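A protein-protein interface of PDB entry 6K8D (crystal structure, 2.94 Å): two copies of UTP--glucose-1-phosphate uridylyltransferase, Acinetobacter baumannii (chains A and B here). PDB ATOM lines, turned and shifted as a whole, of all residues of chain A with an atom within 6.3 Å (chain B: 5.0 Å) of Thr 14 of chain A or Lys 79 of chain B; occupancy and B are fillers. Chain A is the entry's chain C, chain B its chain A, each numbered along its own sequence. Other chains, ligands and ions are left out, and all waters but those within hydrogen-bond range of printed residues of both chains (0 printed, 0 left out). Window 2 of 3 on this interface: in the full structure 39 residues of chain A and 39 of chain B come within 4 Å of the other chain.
OG1 of Thr 14 of chain A is in hydrogen-bond range of NZ of Lys 81 of chain B (3.3 Å).
The backbone carbonyl oxygen (O) of Leu 72 of chain B sits at hydrogen-bond distance from the side-chain hydroxyl (OG1) of Thr 75 of chain B (2.9 Å).
The backbone NH (N) of Lys 81 of chain B is in hydrogen-bond range of the backbone carbonyl oxygen (O) of Leu 76 of chain B, 3.2 Å away.
Among the printed residues, merely in contact across the chains: Thr 14 of chain A with Leu 84 of chain B (3.7 Å), Thr 14 of chain A with Lys 79 of chain B (3.8 Å), Thr 14 of chain A with Leu 72 of chain B (3.9 Å), Leu 12 of chain A with Thr 75 of chain B (3.9 Å) and Thr 14 of chain A with Leu 76 of chain B (3.96 Å).
Printed residues of chain B within 4 Å of Leu 12 of chain A: Thr 75 (3.9 Å).
Thr 14 of chain A touches just these residues of chain B: Leu 72 (3.9 Å), Leu 76 (3.96 Å), Lys 79 (3.8 Å), Lys 81 (3.3 Å) and Leu 84 (3.7 Å).
Printed residues of chain A within 4 Å of Leu 72 of chain B: Thr 14.
Of the printed residues of chain A, Thr 75 of chain B touches Leu 12.
Lys 79 of chain B touches just one residue of chain A: Thr 14 (3.8 Å).
Printed residues of chain A within 4 Å of Lys 81 of chain B: Thr 14 (3.3 Å).
The nearest residue of chain B that does not touch Thr 14 of chain A is Thr 75 of chain B (4.4 Å).
The nearest residue of chain A that does not touch Lys 79 of chain B is Glu 230 of chain A (5.3 Å).
Printed residues of chain A that touch a printed residue of chain B: Leu 12 and Thr 14.
Of the 9 printed residues of chain B, 6 touch a printed residue of chain A.
Among the printed residues, no Asp or Glu carboxylate lies within 4 Å of a Lys or Arg side-chain nitrogen of the other chain.
No position is printed for both chains.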
ATOM      1  N   LEU A  12       8.310  17.351  28.273  1.00  0.00           N
ATOM      2  CA  LEU A  12       8.640  16.803  26.934  1.00  0.00           C
ATOM      3  C   LEU A  12       9.026  17.995  26.054  1.00  0.00           C
ATOM      4  O   LEU A  12       8.892  19.137  26.517  1.00  0.00           O
ATOM      5  CB  LEU A  12       7.438  16.031  26.389  1.00  0.00           C
ATOM      6  CG  LEU A  12       7.155  14.673  27.043  1.00  0.00           C
ATOM      7  CD1 LEU A  12       7.615  14.601  28.493  1.00  0.00           C
ATOM      8  CD2 LEU A  12       5.672  14.345  26.964  1.00  0.00           C
ATOM      9  N   GLY A  13       9.529  17.774  24.851  1.00  0.00           N
ATOM     10  CA  GLY A  13      10.190  18.865  24.115  1.00  0.00           C
ATOM     11  C   GLY A  13       9.322  19.474  23.034  1.00  0.00           C
ATOM     12  O   GLY A  13       9.918  20.029  22.079  1.00  0.00           O
ATOM     13  N   THR A  14       7.991  19.419  23.189  1.00  0.00           N
ATOM     14  CA  THR A  14       6.997  19.703  22.112  1.00  0.00           C
ATOM     15  C   THR A  14       7.465  20.936  21.327  1.00  0.00           C
ATOM     16  O   THR A  14       7.332  20.918  20.089  1.00  0.00           O
ATOM     17  CB  THR A  14       5.557  19.831  22.647  1.00  0.00           C
ATOM     18  OG1 THR A  14       5.429  20.927  23.557  1.00  0.00           O
ATOM     19  CG2 THR A  14       5.067  18.577  23.339  1.00  0.00           C
ATOM     20  N   ARG A  15       8.022  21.934  22.026  1.00  0.00           N
ATOM     21  CA  ARG A  15       8.654  23.160  21.458  1.00  0.00           C
ATOM     22  C   ARG A  15       9.807  22.792  20.494  1.00  0.00           C
ATOM     23  O   ARG A  15       9.877  23.403  19.406  1.00  0.00           O
ATOM     24  CB  ARG A  15       9.108  24.079  22.602  1.00  0.00           C
ATOM     25  N   PHE A  16      10.700  21.856  20.845  1.00  0.00           N
ATOM     26  CA  PHE A  16      11.776  21.405  19.920  1.00  0.00           C
ATOM     27  C   PHE A  16      11.524  19.967  19.458  1.00  0.00           C
ATOM     28  O   PHE A  16      11.956  19.035  20.150  1.00  0.00           O
ATOM     29  CB  PHE A  16      13.181  21.518  20.523  1.00  0.00           C
ATOM     30  CG  PHE A  16      14.279  21.682  19.491  1.00  0.00           C
ATOM     31  CD1 PHE A  16      14.016  21.584  18.126  1.00  0.00           C
ATOM     32  CD2 PHE A  16      15.583  21.928  19.885  1.00  0.00           C
ATOM     33  CE1 PHE A  16      15.024  21.742  17.188  1.00  0.00           C
ATOM     34  CE2 PHE A  16      16.592  22.073  18.946  1.00  0.00           C
ATOM     35  CZ  PHE A  16      16.311  21.983  17.601  1.00  0.00           C
ATOM     36  N   LEU A  17      10.903  19.819  18.287  1.00  0.00           N
ATOM     37  CA  LEU A  17      10.447  18.524  17.722  1.00  0.00           C
ATOM     38  C   LEU A  17      10.629  18.615  16.209  1.00  0.00           C
ATOM     39  O   LEU A  17      10.458  19.681  15.627  1.00  0.00           O
ATOM     40  CB  LEU A  17       8.980  18.316  18.127  1.00  0.00           C
ATOM     41  CG  LEU A  17       8.600  16.981  18.776  1.00  0.00           C
ATOM     42  CD1 LEU A  17       9.283  16.800  20.114  1.00  0.00           C
ATOM     43  CD2 LEU A  17       7.101  16.879  18.982  1.00  0.00           C
ATOM     44  N   SER A  20      13.492  16.256  19.823  1.00  0.00           N
ATOM     45  CA  SER A  20      13.324  15.590  21.133  1.00  0.00           C
ATOM     46  C   SER A  20      12.338  14.413  21.045  1.00  0.00           C
ATOM     47  O   SER A  20      11.936  13.876  22.107  1.00  0.00           O
ATOM     48  CB  SER A  20      12.894  16.591  22.158  1.00  0.00           C
ATOM     49  OG  SER A  20      11.474  16.675  22.198  1.00  0.00           O
ATOM     50  N   LYS A  25      14.928  16.867  25.255  1.00  0.00           N
ATOM     51  CA  LYS A  25      15.278  18.235  24.779  1.00  0.00           C
ATOM     52  C   LYS A  25      16.616  18.653  25.419  1.00  0.00           C
ATOM     53  O   LYS A  25      17.384  19.411  24.778  1.00  0.00           O
ATOM     54  CB  LYS A  25      14.156  19.224  25.111  1.00  0.00           C
ATOM     55  CG  LYS A  25      13.952  19.518  26.597  1.00  0.00           C
ATOM     56  CD  LYS A  25      12.562  20.067  26.952  1.00  0.00           C
ATOM     57  CE  LYS A  25      12.492  20.847  28.254  1.00  0.00           C
ATOM     58  NZ  LYS A  25      13.069  22.210  28.118  1.00  0.00           N
ATOM     59  N   GLU A 230      -1.633  25.202  35.534  1.00  0.00           N
ATOM     60  CA  GLU A 230      -0.221  24.977  35.926  1.00  0.00           C
ATOM     61  C   GLU A 230       0.085  25.824  37.159  1.00  0.00           C
ATOM     62  O   GLU A 230      -0.258  27.026  37.160  1.00  0.00           O
ATOM     63  CB  GLU A 230       0.744  25.307  34.781  1.00  0.00           C
ATOM     64  CG  GLU A 230       0.675  24.332  33.609  1.00  0.00           C
ATOM     65  CD  GLU A 230       1.969  24.143  32.834  1.00  0.00           C
ATOM     66  OE1 GLU A 230       2.826  25.055  32.881  1.00  0.00           O
ATOM     67  OE2 GLU A 230       2.124  23.077  32.196  1.00  0.00           O
ATOM     68  N   LEU B  72       3.448  11.200  24.055  1.00  0.00           N
ATOM     69  CA  LEU B  72       3.796  12.458  23.338  1.00  0.00           C
ATOM     70  C   LEU B  72       2.663  12.834  22.382  1.00  0.00           C
ATOM     71  O   LEU B  72       2.465  14.047  22.160  1.00  0.00           O
ATOM     72  CB  LEU B  72       5.120  12.317  22.574  1.00  0.00           C
ATOM     73  CG  LEU B  72       5.501  13.509  21.684  1.00  0.00           C
ATOM     74  CD1 LEU B  72       5.535  14.808  22.477  1.00  0.00           C
ATOM     75  CD2 LEU B  72       6.833  13.278  20.974  1.00  0.00           C
ATOM     76  N   THR B  75      -0.163  14.347  24.548  1.00  0.00           N
ATOM     77  CA  THR B  75       0.213  15.706  25.026  1.00  0.00           C
ATOM     78  C   THR B  75       0.056  16.676  23.852  1.00  0.00           C
ATOM     79  O   THR B  75      -0.298  17.840  24.107  1.00  0.00           O
ATOM     80  CB  THR B  75       1.608  15.799  25.668  1.00  0.00           C
ATOM     81  OG1 THR B  75       2.561  15.279  24.745  1.00  0.00           O
ATOM     82  CG2 THR B  75       1.710  15.087  27.003  1.00  0.00           C
ATOM     83  N   LEU B  76       0.282  16.206  22.623  1.00  0.00           N
ATOM     84  CA  LEU B  76       0.185  17.040  21.398  1.00  0.00           C
ATOM     85  C   LEU B  76      -1.286  17.191  20.989  1.00  0.00           C
ATOM     86  O   LEU B  76      -1.543  17.962  20.057  1.00  0.00           O
ATOM     87  CB  LEU B  76       1.010  16.410  20.268  1.00  0.00           C
ATOM     88  CG  LEU B  76       2.520  16.648  20.316  1.00  0.00           C
ATOM     89  CD1 LEU B  76       3.226  15.777  19.292  1.00  0.00           C
ATOM     90  CD2 LEU B  76       2.868  18.108  20.079  1.00  0.00           C
ATOM     91  N   GLU B  77      -2.216  16.485  21.631  1.00  0.00           N
ATOM     92  CA  GLU B  77      -3.674  16.713  21.442  1.00  0.00           C
ATOM     93  C   GLU B  77      -4.201  17.653  22.537  1.00  0.00           C
ATOM     94  O   GLU B  77      -4.959  18.588  22.188  1.00  0.00           O
ATOM     95  CB  GLU B  77      -4.448  15.398  21.479  1.00  0.00           C
ATOM     96  CG  GLU B  77      -4.217  14.506  20.277  1.00  0.00           C
ATOM     97  CD  GLU B  77      -4.832  13.127  20.449  1.00  0.00           C
ATOM     98  OE1 GLU B  77      -4.649  12.279  19.557  1.00  0.00           O
ATOM     99  OE2 GLU B  77      -5.488  12.899  21.484  1.00  0.00           O
ATOM    100  N   GLN B  78      -3.816  17.408  23.801  1.00  0.00           N
ATOM    101  CA  GLN B  78      -4.250  18.186  25.001  1.00  0.00           C
ATOM    102  C   GLN B  78      -3.812  19.651  24.846  1.00  0.00           C
ATOM    103  O   GLN B  78      -4.601  20.528  25.228  1.00  0.00           O
ATOM    104  CB  GLN B  78      -3.776  17.523  26.300  1.00  0.00           C
ATOM    105  CG  GLN B  78      -4.795  16.518  26.841  1.00  0.00           C
ATOM    106  CD  GLN B  78      -4.270  15.499  27.831  1.00  0.00           C
ATOM    107  OE1 GLN B  78      -3.266  15.710  28.516  1.00  0.00           O
ATOM    108  NE2 GLN B  78      -4.974  14.379  27.925  1.00  0.00           N
ATOM    109  N   LYS B  79      -2.614  19.909  24.305  1.00  0.00           N
ATOM    110  CA  LYS B  79      -2.321  21.139  23.514  1.00  0.00           C
ATOM    111  C   LYS B  79      -2.771  20.838  22.080  1.00  0.00           C
ATOM    112  O   LYS B  79      -2.348  19.804  21.552  1.00  0.00           O
ATOM    113  CB  LYS B  79      -0.836  21.524  23.510  1.00  0.00           C
ATOM    114  CG  LYS B  79      -0.130  21.608  24.860  1.00  0.00           C
ATOM    115  CD  LYS B  79       1.170  22.400  24.781  1.00  0.00           C
ATOM    116  CE  LYS B  79       2.323  21.756  25.519  1.00  0.00           C
ATOM    117  NZ  LYS B  79       2.162  21.863  26.987  1.00  0.00           N
ATOM    118  N   LYS B  80      -3.609  21.674  21.470  1.00  0.00           N
ATOM    119  CA  LYS B  80      -4.289  21.328  20.191  1.00  0.00           C
ATOM    120  C   LYS B  80      -3.300  21.540  19.034  1.00  0.00           C
ATOM    121  O   LYS B  80      -3.664  22.230  18.078  1.00  0.00           O
ATOM    122  CB  LYS B  80      -5.596  22.122  20.056  1.00  0.00           C
ATOM    123  N   LYS B  81      -2.107  20.940  19.104  1.00  0.00           N
ATOM    124  CA  LYS B  81      -1.015  21.135  18.110  1.00  0.00           C
ATOM    125  C   LYS B  81      -0.985  19.941  17.147  1.00  0.00           C
ATOM    126  O   LYS B  81      -0.052  19.107  17.264  1.00  0.00           O
ATOM    127  CB  LYS B  81       0.335  21.355  18.804  1.00  0.00           C
ATOM    128  CG  LYS B  81       0.656  22.809  19.136  1.00  0.00           C
ATOM    129  CD  LYS B  81       2.095  23.031  19.544  1.00  0.00           C
ATOM    130  CE  LYS B  81       2.461  22.313  20.829  1.00  0.00           C
ATOM    131  NZ  LYS B  81       3.832  22.650  21.290  1.00  0.00           N
ATOM    132  N   LEU B  84       2.488  19.351  14.490  1.00  0.00           N
ATOM    133  CA  LEU B  84       3.603  18.394  14.704  1.00  0.00           C
ATOM    134  C   LEU B  84       3.043  16.979  14.777  1.00  0.00           C
ATOM    135  O   LEU B  84       3.735  16.068  14.291  1.00  0.00           O
ATOM    136  CB  LEU B  84       4.339  18.721  16.003  1.00  0.00           C
ATOM    137  CG  LEU B  84       4.857  20.151  16.120  1.00  0.00           C
ATOM    138  CD1 LEU B  84       4.718  20.656  17.551  1.00  0.00           C
ATOM    139  CD2 LEU B  84       6.295  20.253  15.627  1.00  0.00           C
